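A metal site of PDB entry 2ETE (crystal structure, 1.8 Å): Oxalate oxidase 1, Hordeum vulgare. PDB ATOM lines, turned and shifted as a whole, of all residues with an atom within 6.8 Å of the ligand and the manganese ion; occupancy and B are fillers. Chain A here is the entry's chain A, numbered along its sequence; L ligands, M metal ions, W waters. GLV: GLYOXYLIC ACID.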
ATOM      1  N   VAL A  56     -12.242  17.356 -24.941  1.00  0.00           N
ATOM      2  CA  VAL A  56     -11.541  16.752 -23.808  1.00  0.00           C
ATOM      3  C   VAL A  56     -10.811  15.493 -24.287  1.00  0.00           C
ATOM      4  O   VAL A  56     -11.436  14.578 -24.835  1.00  0.00           O
ATOM      5  CB  VAL A  56     -12.512  16.375 -22.653  1.00  0.00           C
ATOM      6  CG1 VAL A  56     -11.748  15.732 -21.487  1.00  0.00           C
ATOM      7  CG2 VAL A  56     -13.284  17.605 -22.157  1.00  0.00           C
ATOM      8  N   GLU A  58      -8.998  12.510 -22.709  1.00  0.00           N
ATOM      9  CA  GLU A  58      -8.936  11.930 -21.373  1.00  0.00           C
ATOM     10  C   GLU A  58      -7.698  11.073 -21.151  1.00  0.00           C
ATOM     11  O   GLU A  58      -7.248  10.347 -22.056  1.00  0.00           O
ATOM     12  CB  GLU A  58     -10.205  11.113 -21.067  1.00  0.00           C
ATOM     13  CG  GLU A  58     -11.468  11.964 -21.001  1.00  0.00           C
ATOM     14  CD  GLU A  58     -12.628  11.242 -20.347  1.00  0.00           C
ATOM     15  OE1 GLU A  58     -12.563  10.956 -19.132  1.00  0.00           O
ATOM     16  OE2 GLU A  58     -13.631  10.973 -21.057  1.00  0.00           O
ATOM     17  N   ASN A  75      -6.186  15.044 -17.676  1.00  0.00           N
ATOM     18  CA  ASN A  75      -6.619  15.252 -19.043  1.00  0.00           C
ATOM     19  C   ASN A  75      -6.213  16.590 -19.640  1.00  0.00           C
ATOM     20  O   ASN A  75      -5.710  17.472 -18.939  1.00  0.00           O
ATOM     21  CB  ASN A  75      -8.113  14.954 -19.281  1.00  0.00           C
ATOM     22  CG  ASN A  75      -9.049  15.863 -18.524  1.00  0.00           C
ATOM     23  OD1 ASN A  75     -10.063  15.391 -17.983  1.00  0.00           O
ATOM     24  ND2 ASN A  75      -8.771  17.158 -18.518  1.00  0.00           N
ATOM     25  N   ARG A  76      -6.407  16.689 -20.954  1.00  0.00           N
ATOM     26  CA  ARG A  76      -6.155  17.909 -21.690  1.00  0.00           C
ATOM     27  C   ARG A  76      -7.488  18.398 -22.239  1.00  0.00           C
ATOM     28  O   ARG A  76      -8.326  17.593 -22.649  1.00  0.00           O
ATOM     29  CB  ARG A  76      -5.180  17.620 -22.835  1.00  0.00           C
ATOM     30  CG  ARG A  76      -4.983  18.765 -23.795  1.00  0.00           C
ATOM     31  CD  ARG A  76      -4.018  18.420 -24.911  1.00  0.00           C
ATOM     32  NE  ARG A  76      -3.936  19.518 -25.867  1.00  0.00           N
ATOM     33  CZ  ARG A  76      -2.824  19.896 -26.493  1.00  0.00           C
ATOM     34  NH1 ARG A  76      -1.674  19.246 -26.296  1.00  0.00           N
ATOM     35  NH2 ARG A  76      -2.868  20.920 -27.337  1.00  0.00           N
ATOM     36  N   VAL A  77      -7.687  19.716 -22.240  1.00  0.00           N
ATOM     37  CA  VAL A  77      -8.878  20.305 -22.860  1.00  0.00           C
ATOM     38  C   VAL A  77      -8.448  21.450 -23.776  1.00  0.00           C
ATOM     39  O   VAL A  77      -7.738  22.360 -23.354  1.00  0.00           O
ATOM     40  CB  VAL A  77      -9.916  20.805 -21.809  1.00  0.00           C
ATOM     41  CG1 VAL A  77     -11.216  21.226 -22.486  1.00  0.00           C
ATOM     42  CG2 VAL A  77     -10.209  19.717 -20.765  1.00  0.00           C
ATOM     43  N   PHE A  79      -9.772  24.476 -26.628  1.00  0.00           N
ATOM     44  CA  PHE A  79     -10.928  25.371 -26.805  1.00  0.00           C
ATOM     45  C   PHE A  79     -10.811  26.209 -28.071  1.00  0.00           C
ATOM     46  O   PHE A  79      -9.800  26.878 -28.282  1.00  0.00           O
ATOM     47  CB  PHE A  79     -11.019  26.383 -25.648  1.00  0.00           C
ATOM     48  CG  PHE A  79     -11.155  25.783 -24.284  1.00  0.00           C
ATOM     49  CD1 PHE A  79     -12.385  25.815 -23.625  1.00  0.00           C
ATOM     50  CD2 PHE A  79     -10.050  25.257 -23.609  1.00  0.00           C
ATOM     51  CE1 PHE A  79     -12.520  25.288 -22.341  1.00  0.00           C
ATOM     52  CE2 PHE A  79     -10.177  24.735 -22.324  1.00  0.00           C
ATOM     53  CZ  PHE A  79     -11.416  24.747 -21.685  1.00  0.00           C
ATOM     54  N   ASN A  85     -16.036  24.628 -21.925  1.00  0.00           N
ATOM     55  CA  ASN A  85     -16.151  23.345 -21.241  1.00  0.00           C
ATOM     56  C   ASN A  85     -17.224  23.621 -20.182  1.00  0.00           C
ATOM     57  O   ASN A  85     -16.948  24.263 -19.164  1.00  0.00           O
ATOM     58  CB  ASN A  85     -14.809  22.940 -20.622  1.00  0.00           C
ATOM     59  CG  ASN A  85     -14.782  21.479 -20.150  1.00  0.00           C
ATOM     60  OD1 ASN A  85     -15.551  20.636 -20.626  1.00  0.00           O
ATOM     61  ND2 ASN A  85     -13.872  21.181 -19.225  1.00  0.00           N
ATOM     62  N   HIS A  88     -19.880  21.699 -14.989  1.00  0.00           N
ATOM     63  CA  HIS A  88     -19.772  20.263 -14.743  1.00  0.00           C
ATOM     64  C   HIS A  88     -19.225  19.966 -13.348  1.00  0.00           C
ATOM     65  O   HIS A  88     -18.739  20.872 -12.658  1.00  0.00           O
ATOM     66  CB  HIS A  88     -18.932  19.579 -15.836  1.00  0.00           C
ATOM     67  CG  HIS A  88     -17.478  19.950 -15.821  1.00  0.00           C
ATOM     68  ND1 HIS A  88     -16.983  21.067 -16.452  1.00  0.00           N
ATOM     69  CD2 HIS A  88     -16.402  19.322 -15.287  1.00  0.00           C
ATOM     70  CE1 HIS A  88     -15.679  21.123 -16.296  1.00  0.00           C
ATOM     71  NE2 HIS A  88     -15.294  20.071 -15.593  1.00  0.00           N
ATOM     72  N   ILE A  89     -19.337  18.699 -12.944  1.00  0.00           N
ATOM     73  CA  ILE A  89     -18.904  18.241 -11.627  1.00  0.00           C
ATOM     74  C   ILE A  89     -18.089  16.959 -11.770  1.00  0.00           C
ATOM     75  O   ILE A  89     -18.410  16.129 -12.631  1.00  0.00           O
ATOM     76  CB  ILE A  89     -20.127  17.955 -10.697  1.00  0.00           C
ATOM     77  CG1 ILE A  89     -20.757  19.263 -10.203  1.00  0.00           C
ATOM     78  CG2 ILE A  89     -19.742  17.098  -9.483  1.00  0.00           C
ATOM     79  CD1 ILE A  89     -21.926  19.737 -11.022  1.00  0.00           C
ATOM     80  N   HIS A  90     -17.040  16.819 -10.958  1.00  0.00           N
ATOM     81  CA  HIS A  90     -16.335  15.543 -10.806  1.00  0.00           C
ATOM     82  C   HIS A  90     -16.776  14.905  -9.490  1.00  0.00           C
ATOM     83  O   HIS A  90     -16.467  15.412  -8.410  1.00  0.00           O
ATOM     84  CB  HIS A  90     -14.819  15.733 -10.878  1.00  0.00           C
ATOM     85  CG  HIS A  90     -14.383  16.472 -12.094  1.00  0.00           C
ATOM     86  ND1 HIS A  90     -14.457  15.929 -13.361  1.00  0.00           N
ATOM     87  CD2 HIS A  90     -13.907  17.731 -12.257  1.00  0.00           C
ATOM     88  CE1 HIS A  90     -14.053  16.820 -14.249  1.00  0.00           C
ATOM     89  NE2 HIS A  90     -13.706  17.920 -13.607  1.00  0.00           N
ATOM     90  N   GLU A  95      -9.803  18.670  -8.641  1.00  0.00           N
ATOM     91  CA  GLU A  95      -9.082  18.972  -9.880  1.00  0.00           C
ATOM     92  C   GLU A  95      -8.085  20.097  -9.642  1.00  0.00           C
ATOM     93  O   GLU A  95      -8.391  21.068  -8.948  1.00  0.00           O
ATOM     94  CB  GLU A  95     -10.074  19.377 -10.980  1.00  0.00           C
ATOM     95  CG  GLU A  95      -9.446  19.780 -12.316  1.00  0.00           C
ATOM     96  CD  GLU A  95     -10.485  20.178 -13.358  1.00  0.00           C
ATOM     97  OE1 GLU A  95     -11.664  19.792 -13.217  1.00  0.00           O
ATOM     98  OE2 GLU A  95     -10.119  20.889 -14.318  1.00  0.00           O
ATOM     99  N   PHE A 129      -5.358  26.862 -11.263  1.00  0.00           N
ATOM    100  CA  PHE A 129      -6.623  26.885 -10.526  1.00  0.00           C
ATOM    101  C   PHE A 129      -6.840  25.552  -9.828  1.00  0.00           C
ATOM    102  O   PHE A 129      -6.271  24.525 -10.246  1.00  0.00           O
ATOM    103  CB  PHE A 129      -7.808  27.204 -11.477  1.00  0.00           C
ATOM    104  CG  PHE A 129      -7.930  26.247 -12.636  1.00  0.00           C
ATOM    105  CD1 PHE A 129      -8.672  25.064 -12.509  1.00  0.00           C
ATOM    106  CD2 PHE A 129      -7.321  26.529 -13.862  1.00  0.00           C
ATOM    107  CE1 PHE A 129      -8.789  24.176 -13.578  1.00  0.00           C
ATOM    108  CE2 PHE A 129      -7.437  25.641 -14.941  1.00  0.00           C
ATOM    109  CZ  PHE A 129      -8.172  24.465 -14.794  1.00  0.00           C
ATOM    110  N   ILE A 131     -10.103  23.103  -8.026  1.00  0.00           N
ATOM    111  CA  ILE A 131     -11.548  22.880  -7.920  1.00  0.00           C
ATOM    112  C   ILE A 131     -11.841  21.778  -6.916  1.00  0.00           C
ATOM    113  O   ILE A 131     -11.582  20.604  -7.201  1.00  0.00           O
ATOM    114  CB  ILE A 131     -12.164  22.372  -9.258  1.00  0.00           C
ATOM    115  CG1 ILE A 131     -11.520  23.014 -10.503  1.00  0.00           C
ATOM    116  CG2 ILE A 131     -13.709  22.458  -9.209  1.00  0.00           C
ATOM    117  CD1 ILE A 131     -11.938  24.419 -10.807  1.00  0.00           C
ATOM    118  N   HIS A 137     -18.329  23.763 -11.822  1.00  0.00           N
ATOM    119  CA  HIS A 137     -17.300  24.641 -12.393  1.00  0.00           C
ATOM    120  C   HIS A 137     -17.315  24.615 -13.927  1.00  0.00           C
ATOM    121  O   HIS A 137     -17.898  23.715 -14.532  1.00  0.00           O
ATOM    122  CB  HIS A 137     -15.897  24.278 -11.850  1.00  0.00           C
ATOM    123  CG  HIS A 137     -15.436  22.901 -12.204  1.00  0.00           C
ATOM    124  ND1 HIS A 137     -15.967  21.768 -11.625  1.00  0.00           N
ATOM    125  CD2 HIS A 137     -14.485  22.470 -13.070  1.00  0.00           C
ATOM    126  CE1 HIS A 137     -15.365  20.700 -12.111  1.00  0.00           C
ATOM    127  NE2 HIS A 137     -14.458  21.091 -12.989  1.00  0.00           N
ATOM    128  N   PHE A 138     -16.675  25.603 -14.550  1.00  0.00           N
ATOM    129  CA  PHE A 138     -16.658  25.714 -16.011  1.00  0.00           C
ATOM    130  C   PHE A 138     -15.424  26.473 -16.490  1.00  0.00           C
ATOM    131  O   PHE A 138     -14.750  27.149 -15.709  1.00  0.00           O
ATOM    132  CB  PHE A 138     -17.931  26.436 -16.496  1.00  0.00           C
ATOM    133  CG  PHE A 138     -18.030  27.870 -16.041  1.00  0.00           C
ATOM    134  CD1 PHE A 138     -17.476  28.901 -16.800  1.00  0.00           C
ATOM    135  CD2 PHE A 138     -18.660  28.192 -14.836  1.00  0.00           C
ATOM    136  CE1 PHE A 138     -17.547  30.232 -16.373  1.00  0.00           C
ATOM    137  CE2 PHE A 138     -18.740  29.516 -14.399  1.00  0.00           C
ATOM    138  CZ  PHE A 138     -18.179  30.539 -15.168  1.00  0.00           C
ATOM    139  N   GLN A 139     -15.143  26.363 -17.796  1.00  0.00           N
ATOM    140  CA  GLN A 139     -14.149  27.211 -18.459  1.00  0.00           C
ATOM    141  C   GLN A 139     -14.727  27.763 -19.755  1.00  0.00           C
ATOM    142  O   GLN A 139     -15.556  27.116 -20.394  1.00  0.00           O
ATOM    143  CB  GLN A 139     -12.845  26.456 -18.733  1.00  0.00           C
ATOM    144  CG  GLN A 139     -12.128  25.905 -17.499  1.00  0.00           C
ATOM    145  CD  GLN A 139     -12.560  24.487 -17.144  1.00  0.00           C
ATOM    146  OE1 GLN A 139     -13.102  23.770 -17.978  1.00  0.00           O
ATOM    147  NE2 GLN A 139     -12.294  24.077 -15.907  1.00  0.00           N
ATOM    148  N   MET A 149      -5.592  23.748 -21.826  1.00  0.00           N
ATOM    149  CA  MET A 149      -5.188  23.544 -20.450  1.00  0.00           C
ATOM    150  C   MET A 149      -4.899  22.067 -20.223  1.00  0.00           C
ATOM    151  O   MET A 149      -5.398  21.199 -20.954  1.00  0.00           O
ATOM    152  CB  MET A 149      -6.274  24.031 -19.472  1.00  0.00           C
ATOM    153  CG  MET A 149      -7.562  23.199 -19.497  1.00  0.00           C
ATOM    154  SD  MET A 149      -8.845  23.843 -18.410  1.00  0.00           S
ATOM    155  CE  MET A 149      -9.934  22.428 -18.334  1.00  0.00           C
ATOM    156  N   VAL A 151      -4.936  19.402 -16.910  1.00  0.00           N
ATOM    157  CA  VAL A 151      -5.399  19.296 -15.525  1.00  0.00           C
ATOM    158  C   VAL A 151      -5.131  17.905 -14.949  1.00  0.00           C
ATOM    159  O   VAL A 151      -5.024  16.922 -15.694  1.00  0.00           O
ATOM    160  CB  VAL A 151      -6.909  19.698 -15.353  1.00  0.00           C
ATOM    161  CG1 VAL A 151      -7.199  21.071 -15.980  1.00  0.00           C
ATOM    162  CG2 VAL A 151      -7.845  18.652 -15.949  1.00  0.00           C
ATOM    163  N   PHE A 153      -6.109  15.154 -11.471  1.00  0.00           N
ATOM    164  CA  PHE A 153      -7.101  14.817 -10.457  1.00  0.00           C
ATOM    165  C   PHE A 153      -6.487  13.898  -9.410  1.00  0.00           C
ATOM    166  O   PHE A 153      -5.554  13.142  -9.716  1.00  0.00           O
ATOM    167  CB  PHE A 153      -8.296  14.076 -11.088  1.00  0.00           C
ATOM    168  CG  PHE A 153      -8.926  14.806 -12.247  1.00  0.00           C
ATOM    169  CD1 PHE A 153      -8.481  14.592 -13.553  1.00  0.00           C
ATOM    170  CD2 PHE A 153      -9.969  15.701 -12.037  1.00  0.00           C
ATOM    171  CE1 PHE A 153      -9.066  15.272 -14.639  1.00  0.00           C
ATOM    172  CE2 PHE A 153     -10.562  16.374 -13.103  1.00  0.00           C
ATOM    173  CZ  PHE A 153     -10.112  16.153 -14.409  1.00  0.00           C
ATOM    174  N   PRO A 158     -12.058  10.191 -12.020  1.00  0.00           N
ATOM    175  CA  PRO A 158     -12.815  11.252 -11.353  1.00  0.00           C
ATOM    176  C   PRO A 158     -14.304  11.276 -11.680  1.00  0.00           C
ATOM    177  O   PRO A 158     -15.119  11.658 -10.836  1.00  0.00           O
ATOM    178  CB  PRO A 158     -12.143  12.542 -11.844  1.00  0.00           C
ATOM    179  CG  PRO A 158     -11.421  12.149 -13.094  1.00  0.00           C
ATOM    180  CD  PRO A 158     -10.999  10.730 -12.890  1.00  0.00           C
ATOM    181  N   GLY A 159     -14.662  10.863 -12.904  1.00  0.00           N
ATOM    182  CA  GLY A 159     -16.033  10.942 -13.394  1.00  0.00           C
ATOM    183  C   GLY A 159     -16.339  12.346 -13.893  1.00  0.00           C
ATOM    184  O   GLY A 159     -15.722  13.313 -13.446  1.00  0.00           O
ATOM    185  N   ILE A 160     -17.271  12.454 -14.829  1.00  0.00           N
ATOM    186  CA  ILE A 160     -17.745  13.776 -15.257  1.00  0.00           C
ATOM    187  C   ILE A 160     -19.257  13.830 -15.365  1.00  0.00           C
ATOM    188  O   ILE A 160     -19.878  13.023 -16.063  1.00  0.00           O
ATOM    189  CB  ILE A 160     -17.038  14.287 -16.558  1.00  0.00           C
ATOM    190  CG1 ILE A 160     -17.450  15.734 -16.862  1.00  0.00           C
ATOM    191  CG2 ILE A 160     -17.338  13.386 -17.737  1.00  0.00           C
ATOM    192  CD1 ILE A 160     -16.360  16.567 -17.499  1.00  0.00           C
ATOM    193  N   PHE A 162     -21.701  16.349 -16.689  1.00  0.00           N
ATOM    194  CA  PHE A 162     -21.955  17.568 -17.465  1.00  0.00           C
ATOM    195  C   PHE A 162     -23.362  18.053 -17.137  1.00  0.00           C
ATOM    196  O   PHE A 162     -24.333  17.309 -17.314  1.00  0.00           O
ATOM    197  CB  PHE A 162     -21.842  17.315 -18.971  1.00  0.00           C
ATOM    198  CG  PHE A 162     -20.427  17.360 -19.510  1.00  0.00           C
ATOM    199  CD1 PHE A 162     -19.883  16.267 -20.179  1.00  0.00           C
ATOM    200  CD2 PHE A 162     -19.648  18.520 -19.364  1.00  0.00           C
ATOM    201  CE1 PHE A 162     -18.577  16.321 -20.684  1.00  0.00           C
ATOM    202  CE2 PHE A 162     -18.348  18.582 -19.869  1.00  0.00           C
ATOM    203  CZ  PHE A 162     -17.811  17.483 -20.539  1.00  0.00           C
HETATM  204  C1  GLV L   1     -12.291  17.523 -18.142  1.00  0.00           C
HETATM  205  O1  GLV L   1     -12.622  16.432 -17.691  1.00  0.00           O
HETATM  206  C2  GLV L   1     -12.216  18.683 -17.236  1.00  0.00           C
HETATM  207  O2  GLV L   1     -12.010  19.808 -17.674  1.00  0.00           O
HETATM  208  O3  GLV L   1     -12.372  18.538 -15.933  1.00  0.00           O
HETATM  209 MN    MN M   1     -13.409  19.842 -14.361  1.00  0.00          MN
HETATM  210  O   HOH W   1     -14.336  14.187 -18.794  1.00  0.00           O
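The manganese ion is bound by a ring nitrogen (NE2) of His 90 (2.1 Å), the side-chain carboxylate (OE1) of Glu 95 (2.1 Å), a ring nitrogen (NE2) of His 137 (2.1 Å), a ring nitrogen (NE2) of His 88 (2.3 Å) and an oxygen (O3) of the ligand (2.3 Å). The manganese ion has five donor atoms within binding distance.
Merely in contact with the ligand: Val 56 (3.8 Å), Val 77 (3.6 Å), Met 149 (3.4 Å), Phe 153 (3.6 Å) and Ile 160 (3.7 Å). Ten residues have an atom within 4 Å of the ligand: Val 56, Asn 75, Val 77, Asn 85, His 88, His 90, Glu 95, Met 149, Phe 153 and Ile 160.
Along chain A the residues within 4 Å of the manganese ion span positions 88 to 137. The nearest printed residue that does not touch the manganese ion is Gln 139 (4.6 Å).
The backbone carbonyl oxygen of Gln 139 lies within hydrogen-bond range of the backbone NH of Asn 85 (3.0 Å). The backbone NH (N) of Met 149 is in hydrogen-bond range of the backbone carbonyl oxygen (O) of Val 77, 3.0 Å away. O of Glu 95 lies within hydrogen-bond range of N of Ile 131 (2.8 Å). ND1 of His 90 lies within hydrogen-bond range of O of Gly 159 (2.9 Å). N of Val 151 is in hydrogen-bond range of O of Asn 75, 2.9 Å away.
ND2 of Asn 85 lies within hydrogen-bond range of O2 of the ligand (2.8 Å). The side-chain amide oxygen (OD1) of Asn 75 sits close to an oxygen (O1) of the ligand.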
